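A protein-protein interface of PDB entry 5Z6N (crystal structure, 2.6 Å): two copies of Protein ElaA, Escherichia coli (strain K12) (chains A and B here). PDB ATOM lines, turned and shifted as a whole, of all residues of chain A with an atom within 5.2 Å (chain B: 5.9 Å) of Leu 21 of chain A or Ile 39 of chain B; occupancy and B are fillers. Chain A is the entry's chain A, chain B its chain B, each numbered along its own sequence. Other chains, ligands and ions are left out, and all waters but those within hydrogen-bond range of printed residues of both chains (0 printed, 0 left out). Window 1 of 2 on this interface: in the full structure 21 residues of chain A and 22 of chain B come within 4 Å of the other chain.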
ATOM      1  N   LEU A  17      32.382 -11.360   8.949  1.00  0.00           N
ATOM      2  CA  LEU A  17      31.146 -12.033   9.341  1.00  0.00           C
ATOM      3  C   LEU A  17      30.314 -11.154  10.273  1.00  0.00           C
ATOM      4  O   LEU A  17      29.097 -11.011  10.095  1.00  0.00           O
ATOM      5  CB  LEU A  17      31.483 -13.375   9.999  1.00  0.00           C
ATOM      6  CG  LEU A  17      30.403 -14.441  10.255  1.00  0.00           C
ATOM      7  CD1 LEU A  17      29.622 -14.161  11.527  1.00  0.00           C
ATOM      8  CD2 LEU A  17      29.457 -14.579   9.069  1.00  0.00           C
ATOM      9  N   TYR A  18      30.963 -10.551  11.272  1.00  0.00           N
ATOM     10  CA  TYR A  18      30.280  -9.653  12.197  1.00  0.00           C
ATOM     11  C   TYR A  18      29.660  -8.471  11.461  1.00  0.00           C
ATOM     12  O   TYR A  18      28.532  -8.059  11.757  1.00  0.00           O
ATOM     13  CB  TYR A  18      31.275  -9.169  13.258  1.00  0.00           C
ATOM     14  CG  TYR A  18      30.669  -8.485  14.462  1.00  0.00           C
ATOM     15  CD1 TYR A  18      30.291  -9.220  15.579  1.00  0.00           C
ATOM     16  CD2 TYR A  18      30.487  -7.106  14.490  1.00  0.00           C
ATOM     17  CE1 TYR A  18      29.748  -8.607  16.690  1.00  0.00           C
ATOM     18  CE2 TYR A  18      29.938  -6.481  15.599  1.00  0.00           C
ATOM     19  CZ  TYR A  18      29.576  -7.238  16.697  1.00  0.00           C
ATOM     20  OH  TYR A  18      29.023  -6.636  17.805  1.00  0.00           O
ATOM     21  N   ALA A  19      30.383  -7.923  10.481  1.00  0.00           N
ATOM     22  CA  ALA A  19      29.956  -6.684   9.842  1.00  0.00           C
ATOM     23  C   ALA A  19      28.694  -6.880   9.005  1.00  0.00           C
ATOM     24  O   ALA A  19      27.784  -6.043   9.044  1.00  0.00           O
ATOM     25  CB  ALA A  19      31.092  -6.123   8.987  1.00  0.00           C
ATOM     26  N   LEU A  20      28.615  -7.975   8.242  1.00  0.00           N
ATOM     27  CA  LEU A  20      27.462  -8.155   7.362  1.00  0.00           C
ATOM     28  C   LEU A  20      26.207  -8.509   8.157  1.00  0.00           C
ATOM     29  O   LEU A  20      25.107  -8.065   7.812  1.00  0.00           O
ATOM     30  CB  LEU A  20      27.767  -9.202   6.279  1.00  0.00           C
ATOM     31  CG  LEU A  20      28.138 -10.664   6.533  1.00  0.00           C
ATOM     32  CD1 LEU A  20      26.900 -11.539   6.452  1.00  0.00           C
ATOM     33  CD2 LEU A  20      29.176 -11.116   5.514  1.00  0.00           C
ATOM     34  N   LEU A  21      26.354  -9.283   9.236  1.00  0.00           N
ATOM     35  CA  LEU A  21      25.241  -9.490  10.162  1.00  0.00           C
ATOM     36  C   LEU A  21      24.837  -8.185  10.845  1.00  0.00           C
ATOM     37  O   LEU A  21      23.644  -7.909  11.020  1.00  0.00           O
ATOM     38  CB  LEU A  21      25.615 -10.532  11.218  1.00  0.00           C
ATOM     39  CG  LEU A  21      25.496 -12.040  10.975  1.00  0.00           C
ATOM     40  CD1 LEU A  21      26.040 -12.467   9.640  1.00  0.00           C
ATOM     41  CD2 LEU A  21      26.210 -12.789  12.085  1.00  0.00           C
ATOM     42  N   GLN A  22      25.823  -7.385  11.258  1.00  0.00           N
ATOM     43  CA  GLN A  22      25.547  -6.114  11.924  1.00  0.00           C
ATOM     44  C   GLN A  22      24.717  -5.196  11.038  1.00  0.00           C
ATOM     45  O   GLN A  22      23.744  -4.582  11.494  1.00  0.00           O
ATOM     46  CB  GLN A  22      26.865  -5.439  12.305  1.00  0.00           C
ATOM     47  CG  GLN A  22      26.732  -4.135  13.046  1.00  0.00           C
ATOM     48  CD  GLN A  22      28.068  -3.419  13.170  1.00  0.00           C
ATOM     49  OE1 GLN A  22      28.383  -2.852  14.208  1.00  0.00           O
ATOM     50  NE2 GLN A  22      28.858  -3.449  12.111  1.00  0.00           N
ATOM     51  N   LEU A  23      25.099  -5.081   9.763  1.00  0.00           N
ATOM     52  CA  LEU A  23      24.327  -4.281   8.817  1.00  0.00           C
ATOM     53  C   LEU A  23      22.979  -4.928   8.513  1.00  0.00           C
ATOM     54  O   LEU A  23      21.974  -4.228   8.342  1.00  0.00           O
ATOM     55  CB  LEU A  23      25.136  -4.084   7.537  1.00  0.00           C
ATOM     56  CG  LEU A  23      24.447  -3.425   6.346  1.00  0.00           C
ATOM     57  CD1 LEU A  23      24.210  -1.932   6.593  1.00  0.00           C
ATOM     58  CD2 LEU A  23      25.275  -3.656   5.088  1.00  0.00           C
ATOM     59  N   ARG A  24      22.936  -6.262   8.448  1.00  0.00           N
ATOM     60  CA  ARG A  24      21.674  -6.952   8.190  1.00  0.00           C
ATOM     61  C   ARG A  24      20.692  -6.748   9.336  1.00  0.00           C
ATOM     62  O   ARG A  24      19.506  -6.477   9.111  1.00  0.00           O
ATOM     63  CB  ARG A  24      21.925  -8.441   7.957  1.00  0.00           C
ATOM     64  CG  ARG A  24      21.821  -8.861   6.503  1.00  0.00           C
ATOM     65  CD  ARG A  24      22.593 -10.144   6.251  1.00  0.00           C
ATOM     66  NE  ARG A  24      22.091 -11.256   7.050  1.00  0.00           N
ATOM     67  CZ  ARG A  24      22.610 -12.478   7.031  1.00  0.00           C
ATOM     68  NH1 ARG A  24      22.093 -13.432   7.795  1.00  0.00           N
ATOM     69  NH2 ARG A  24      23.647 -12.747   6.250  1.00  0.00           N
ATOM     70  N   CYS A  25      21.165  -6.892  10.576  1.00  0.00           N
ATOM     71  CA  CYS A  25      20.331  -6.550  11.723  1.00  0.00           C
ATOM     72  C   CYS A  25      19.895  -5.092  11.654  1.00  0.00           C
ATOM     73  O   CYS A  25      18.732  -4.762  11.913  1.00  0.00           O
ATOM     74  CB  CYS A  25      21.089  -6.828  13.024  1.00  0.00           C
ATOM     75  SG  CYS A  25      20.131  -6.542  14.534  1.00  0.00           S
ATOM     76  N   ALA A  26      20.818  -4.207  11.269  1.00  0.00           N
ATOM     77  CA  ALA A  26      20.520  -2.778  11.253  1.00  0.00           C
ATOM     78  C   ALA A  26      19.543  -2.413  10.145  1.00  0.00           C
ATOM     79  O   ALA A  26      18.892  -1.366  10.211  1.00  0.00           O
ATOM     80  CB  ALA A  26      21.809  -1.971  11.110  1.00  0.00           C
ATOM     81  N   ASP A  38      17.166 -13.232  11.276  1.00  0.00           N
ATOM     82  CA  ASP A  38      18.019 -12.919  10.132  1.00  0.00           C
ATOM     83  C   ASP A  38      19.166 -13.914  10.015  1.00  0.00           C
ATOM     84  O   ASP A  38      19.503 -14.359   8.911  1.00  0.00           O
ATOM     85  CB  ASP A  38      18.561 -11.493  10.251  1.00  0.00           C
ATOM     86  CG  ASP A  38      19.662 -11.202   9.246  1.00  0.00           C
ATOM     87  OD1 ASP A  38      19.349 -10.998   8.054  1.00  0.00           O
ATOM     88  OD2 ASP A  38      20.845 -11.179   9.646  1.00  0.00           O
ATOM     89  N   ILE A  39      19.771 -14.274  11.142  1.00  0.00           N
ATOM     90  CA  ILE A  39      20.864 -15.234  11.173  1.00  0.00           C
ATOM     91  C   ILE A  39      20.144 -16.576  11.094  1.00  0.00           C
ATOM     92  O   ILE A  39      19.723 -17.133  12.115  1.00  0.00           O
ATOM     93  CB  ILE A  39      21.695 -15.050  12.454  1.00  0.00           C
ATOM     94  CG1 ILE A  39      21.975 -13.563  12.673  1.00  0.00           C
ATOM     95  CG2 ILE A  39      23.008 -15.764  12.348  1.00  0.00           C
ATOM     96  CD1 ILE A  39      22.239 -13.187  14.106  1.00  0.00           C
ATOM     97  N   ASP A  43      24.195 -18.872   5.705  1.00  0.00           N
ATOM     98  CA  ASP A  43      25.337 -18.049   5.332  1.00  0.00           C
ATOM     99  C   ASP A  43      26.609 -18.861   5.103  1.00  0.00           C
ATOM    100  O   ASP A  43      27.412 -18.512   4.232  1.00  0.00           O
ATOM    101  CB  ASP A  43      25.580 -16.991   6.412  1.00  0.00           C
ATOM    102  CG  ASP A  43      24.376 -16.101   6.634  1.00  0.00           C
ATOM    103  OD1 ASP A  43      23.879 -15.511   5.652  1.00  0.00           O
ATOM    104  OD2 ASP A  43      23.915 -16.001   7.788  1.00  0.00           O
ATOM    105  N   LEU B  17      31.440 -17.406  16.395  1.00  0.00           N
ATOM    106  CA  LEU B  17      30.741 -16.125  16.375  1.00  0.00           C
ATOM    107  C   LEU B  17      29.339 -16.276  15.803  1.00  0.00           C
ATOM    108  O   LEU B  17      28.372 -15.724  16.343  1.00  0.00           O
ATOM    109  CB  LEU B  17      31.535 -15.100  15.565  1.00  0.00           C
ATOM    110  CG  LEU B  17      30.787 -13.780  15.378  1.00  0.00           C
ATOM    111  CD1 LEU B  17      30.498 -13.147  16.731  1.00  0.00           C
ATOM    112  CD2 LEU B  17      31.554 -12.826  14.475  1.00  0.00           C
ATOM    113  N   TYR B  18      29.211 -17.021  14.703  1.00  0.00           N
ATOM    114  CA  TYR B  18      27.903 -17.214  14.089  1.00  0.00           C
ATOM    115  C   TYR B  18      26.915 -17.841  15.061  1.00  0.00           C
ATOM    116  O   TYR B  18      25.736 -17.470  15.087  1.00  0.00           O
ATOM    117  CB  TYR B  18      28.026 -18.083  12.840  1.00  0.00           C
ATOM    118  CG  TYR B  18      26.805 -18.002  11.959  1.00  0.00           C
ATOM    119  CD1 TYR B  18      26.619 -16.920  11.112  1.00  0.00           C
ATOM    120  CD2 TYR B  18      25.825 -18.988  11.991  1.00  0.00           C
ATOM    121  CE1 TYR B  18      25.508 -16.830  10.302  1.00  0.00           C
ATOM    122  CE2 TYR B  18      24.702 -18.905  11.185  1.00  0.00           C
ATOM    123  CZ  TYR B  18      24.552 -17.825  10.338  1.00  0.00           C
ATOM    124  OH  TYR B  18      23.439 -17.724   9.532  1.00  0.00           O
ATOM    125  N   LEU B  21      25.631 -15.134  18.007  1.00  0.00           N
ATOM    126  CA  LEU B  21      24.729 -14.084  17.546  1.00  0.00           C
ATOM    127  C   LEU B  21      23.404 -14.673  17.073  1.00  0.00           C
ATOM    128  O   LEU B  21      22.341 -14.074  17.277  1.00  0.00           O
ATOM    129  CB  LEU B  21      25.385 -13.272  16.431  1.00  0.00           C
ATOM    130  CG  LEU B  21      26.717 -12.595  16.759  1.00  0.00           C
ATOM    131  CD1 LEU B  21      27.347 -12.047  15.492  1.00  0.00           C
ATOM    132  CD2 LEU B  21      26.511 -11.495  17.779  1.00  0.00           C
ATOM    133  N   ARG B  24      21.614 -15.380  20.184  1.00  0.00           N
ATOM    134  CA  ARG B  24      21.191 -14.106  20.756  1.00  0.00           C
ATOM    135  C   ARG B  24      20.014 -13.528  19.983  1.00  0.00           C
ATOM    136  O   ARG B  24      19.046 -13.039  20.578  1.00  0.00           O
ATOM    137  CB  ARG B  24      22.359 -13.120  20.772  1.00  0.00           C
ATOM    138  CG  ARG B  24      23.229 -13.194  22.016  1.00  0.00           C
ATOM    139  CD  ARG B  24      24.645 -12.764  21.706  1.00  0.00           C
ATOM    140  NE  ARG B  24      24.712 -11.358  21.317  1.00  0.00           N
ATOM    141  CZ  ARG B  24      25.843 -10.669  21.211  1.00  0.00           C
ATOM    142  NH1 ARG B  24      25.814  -9.395  20.850  1.00  0.00           N
ATOM    143  NH2 ARG B  24      27.004 -11.251  21.473  1.00  0.00           N
ATOM    144  N   TYR B  36      15.679  -4.741  17.758  1.00  0.00           N
ATOM    145  CA  TYR B  36      16.687  -3.868  18.346  1.00  0.00           C
ATOM    146  C   TYR B  36      18.012  -4.297  17.724  1.00  0.00           C
ATOM    147  O   TYR B  36      18.085  -5.266  16.962  1.00  0.00           O
ATOM    148  CB  TYR B  36      16.774  -3.802  19.880  1.00  0.00           C
ATOM    149  CG  TYR B  36      17.628  -4.872  20.528  1.00  0.00           C
ATOM    150  CD1 TYR B  36      17.181  -6.184  20.626  1.00  0.00           C
ATOM    151  CD2 TYR B  36      18.876  -4.565  21.059  1.00  0.00           C
ATOM    152  CE1 TYR B  36      17.963  -7.166  21.227  1.00  0.00           C
ATOM    153  CE2 TYR B  36      19.661  -5.536  21.660  1.00  0.00           C
ATOM    154  CZ  TYR B  36      19.200  -6.834  21.741  1.00  0.00           C
ATOM    155  OH  TYR B  36      19.980  -7.802  22.337  1.00  0.00           O
ATOM    156  N   GLN B  37      19.072  -3.552  18.050  1.00  0.00           N
ATOM    157  CA  GLN B  37      20.405  -3.788  17.491  1.00  0.00           C
ATOM    158  C   GLN B  37      21.191  -4.693  18.437  1.00  0.00           C
ATOM    159  O   GLN B  37      21.959  -4.245  19.292  1.00  0.00           O
ATOM    160  CB  GLN B  37      21.122  -2.463  17.252  1.00  0.00           C
ATOM    161  CG  GLN B  37      22.434  -2.587  16.501  1.00  0.00           C
ATOM    162  CD  GLN B  37      22.237  -2.878  15.026  1.00  0.00           C
ATOM    163  OE1 GLN B  37      21.427  -2.233  14.357  1.00  0.00           O
ATOM    164  NE2 GLN B  37      22.981  -3.852  14.510  1.00  0.00           N
ATOM    165  N   ASP B  38      20.996  -6.002  18.267  1.00  0.00           N
ATOM    166  CA  ASP B  38      21.688  -6.967  19.119  1.00  0.00           C
ATOM    167  C   ASP B  38      23.190  -6.976  18.862  1.00  0.00           C
ATOM    168  O   ASP B  38      23.977  -7.243  19.778  1.00  0.00           O
ATOM    169  CB  ASP B  38      21.108  -8.366  18.906  1.00  0.00           C
ATOM    170  CG  ASP B  38      21.943  -9.443  19.568  1.00  0.00           C
ATOM    171  OD1 ASP B  38      22.182  -9.337  20.789  1.00  0.00           O
ATOM    172  OD2 ASP B  38      22.374 -10.385  18.868  1.00  0.00           O
ATOM    173  N   ILE B  39      23.599  -6.685  17.633  1.00  0.00           N
ATOM    174  CA  ILE B  39      25.001  -6.743  17.230  1.00  0.00           C
ATOM    175  C   ILE B  39      25.512  -5.305  17.274  1.00  0.00           C
ATOM    176  O   ILE B  39      25.389  -4.542  16.315  1.00  0.00           O
ATOM    177  CB  ILE B  39      25.158  -7.392  15.857  1.00  0.00           C
ATOM    178  CG1 ILE B  39      24.657  -8.838  15.911  1.00  0.00           C
ATOM    179  CG2 ILE B  39      26.590  -7.356  15.396  1.00  0.00           C
ATOM    180  CD1 ILE B  39      24.128  -9.359  14.594  1.00  0.00           C
ATOM    181  N   ASP B  40      26.095  -4.930  18.415  1.00  0.00           N
ATOM    182  CA  ASP B  40      26.367  -3.535  18.732  1.00  0.00           C
ATOM    183  C   ASP B  40      27.843  -3.162  18.678  1.00  0.00           C
ATOM    184  O   ASP B  40      28.179  -2.002  18.945  1.00  0.00           O
ATOM    185  CB  ASP B  40      25.811  -3.196  20.121  1.00  0.00           C
ATOM    186  CG  ASP B  40      26.327  -4.130  21.205  1.00  0.00           C
ATOM    187  OD1 ASP B  40      27.254  -4.924  20.936  1.00  0.00           O
ATOM    188  OD2 ASP B  40      25.804  -4.067  22.337  1.00  0.00           O
ATOM    189  N   GLY B  41      28.730  -4.098  18.355  1.00  0.00           N
ATOM    190  CA  GLY B  41      30.149  -3.791  18.308  1.00  0.00           C
ATOM    191  C   GLY B  41      30.915  -4.298  19.514  1.00  0.00           C
ATOM    192  O   GLY B  41      32.048  -4.771  19.386  1.00  0.00           O
ATOM    193  N   ASP B  43      31.361  -6.761  20.995  1.00  0.00           N
ATOM    194  CA  ASP B  43      31.803  -8.148  21.062  1.00  0.00           C
ATOM    195  C   ASP B  43      33.262  -8.374  20.691  1.00  0.00           C
ATOM    196  O   ASP B  43      33.900  -9.267  21.258  1.00  0.00           O
ATOM    197  CB  ASP B  43      30.904  -9.006  20.168  1.00  0.00           C
ATOM    198  CG  ASP B  43      29.468  -9.032  20.650  1.00  0.00           C
ATOM    199  OD1 ASP B  43      29.204  -9.681  21.684  1.00  0.00           O
ATOM    200  OD2 ASP B  43      28.607  -8.405  19.998  1.00  0.00           O
ATOM    201  N   ARG B  79      23.663 -10.349  28.169  1.00  0.00           N
ATOM    202  CA  ARG B  79      23.284 -11.310  27.125  1.00  0.00           C
ATOM    203  C   ARG B  79      23.102 -12.722  27.684  1.00  0.00           C
ATOM    204  O   ARG B  79      23.328 -13.714  26.984  1.00  0.00           O
ATOM    205  CB  ARG B  79      24.296 -11.317  25.972  1.00  0.00           C
ATOM    206  CG  ARG B  79      24.456  -9.992  25.261  1.00  0.00           C
ATOM    207  CD  ARG B  79      23.109  -9.416  24.863  1.00  0.00           C
ATOM    208  NE  ARG B  79      23.178  -8.668  23.615  1.00  0.00           N
ATOM    209  CZ  ARG B  79      23.452  -7.369  23.549  1.00  0.00           C
ATOM    210  NH1 ARG B  79      23.492  -6.755  22.378  1.00  0.00           N
ATOM    211  NH2 ARG B  79      23.714  -6.681  24.649  1.00  0.00           N
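Among the printed residues, merely in contact across the chains: Tyr 18 of chain A with Ile 39 of chain B (3.3 Å), Ile 39 of chain A with Tyr 18 of chain B (3.3 Å), Ala 26 of chain A with Gln 37 of chain B (3.3 Å), Ile 39 of chain A with Leu 21 of chain B (3.3 Å), Gln 22 of chain A with Ile 39 of chain B (3.6 Å), Leu 21 of chain A with Leu 21 of chain B (3.7 Å), Leu 17 of chain A with Leu 17 of chain B (3.8 Å), Cys 25 of chain A with Gln 37 of chain B (3.8 Å), Tyr 18 of chain A with Leu 17 of chain B (3.9 Å), Cys 25 of chain A with Asp 38 of chain B (3.9 Å) and Leu 21 of chain A with Ile 39 of chain B (3.9 Å).
Hydrophobic or aromatic side chains of chain A within 4 Å of the printed part of chain B: Leu 17, Tyr 18, Leu 21, Ala 26 and Ile 39.
Among the printed residues, no Asp or Glu carboxylate lies within 4 Å of a Lys or Arg side-chain nitrogen of the other chain.
OH of Tyr 18 of chain A lies within hydrogen-bond range of N of Asp 40 of chain B, at 3.4 Å.
The side-chain hydroxyl of Tyr 18 of chain A sits at hydrogen-bond distance from the backbone NH of Gly 41 of chain B (2.6 Å).
The side-chain carboxylate (OD2) of Asp 43 of chain B is in hydrogen-bond range of the side-chain hydroxyl (OH) of Tyr 18 of chain A.
O of Gln 22 of chain A is in hydrogen-bond range of NE2 of Gln 37 of chain B.
The side-chain sulfur of Cys 25 of chain A sits at hydrogen-bond distance from the backbone carbonyl oxygen of Tyr 36 of chain B, at 3.4 Å.
The side-chain carboxylate (OD2) of Asp 43 of chain A lies within hydrogen-bond range of the side-chain hydroxyl (OH) of Tyr 18 of chain B.
Tyr 18 of chain A touches Leu 17 of chain B, but with the chains exchanged Leu 17 of chain A does not touch Tyr 18 of chain B (4.1 Å).
Tyr 18 of chain A touches Ile 39 of chain B, and with the chains exchanged Ile 39 of chain A touches Tyr 18 of chain B.
Tyr 18 of chain A touches Asp 43 of chain B, and with the chains exchanged Asp 43 of chain A touches Tyr 18 of chain B.
Leu 21 of chain B touches its own counterpart, Leu 21 of chain A.
Of the 17 pairs that touch across the chains among the printed residues, 8 have their exchanged pair printed and touching as well.
Leu 21 of chain A touches just these residues of chain B: Leu 21 (3.7 Å) and Ile 39 (3.9 Å).
Of the printed residues of chain B, Leu 17 of chain A touches Leu 17.
Of the printed residues of chain A, Gln 37 of chain B touches Gln 22 (3.2 Å), Cys 25 (3.8 Å) and Ala 26 (3.3 Å).
Printed residues of chain A within 4 Å of Leu 17 of chain B: Leu 17 (3.8 Å) and Tyr 18 (3.9 Å).
Of the printed residues of chain A, Asp 38 of chain B touches Cys 25.
Of the printed residues of chain A, Gly 41 of chain B touches Tyr 18.
Ala 19 of chain A touches none of the printed residues of chain B.
Asp 38 of chain A touches none of the printed residues of chain B.
The nearest printed residue of chain B that does not touch Leu 17 of chain A is Tyr 18 of chain B (4.1 Å).
The side-chain carboxylate (OD1) of Asp 43 of chain A is in salt-bridge range of the guanidinium group (NH2) of Arg 24 of chain A (2.8 Å).
NE of Arg 24 of chain B lies within salt-bridge range of OD1 of Asp 38 of chain B, at 3.3 Å.
The guanidinium group of Arg 24 of chain B lies within salt-bridge range of the side-chain carboxylate of Asp 43 of chain B (2.7 Å).
O of Ile 39 of chain B is in hydrogen-bond range of NE2 of Gln 37 of chain B (3.1 Å).
OD1 of Asp 38 of chain B lies within salt-bridge range of NE of Arg 79 of chain B (3.1 Å).
The side-chain carboxylate of Asp 40 of chain B is in salt-bridge range of the guanidinium group of Arg 79 of chain B, 3.5 Å away.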
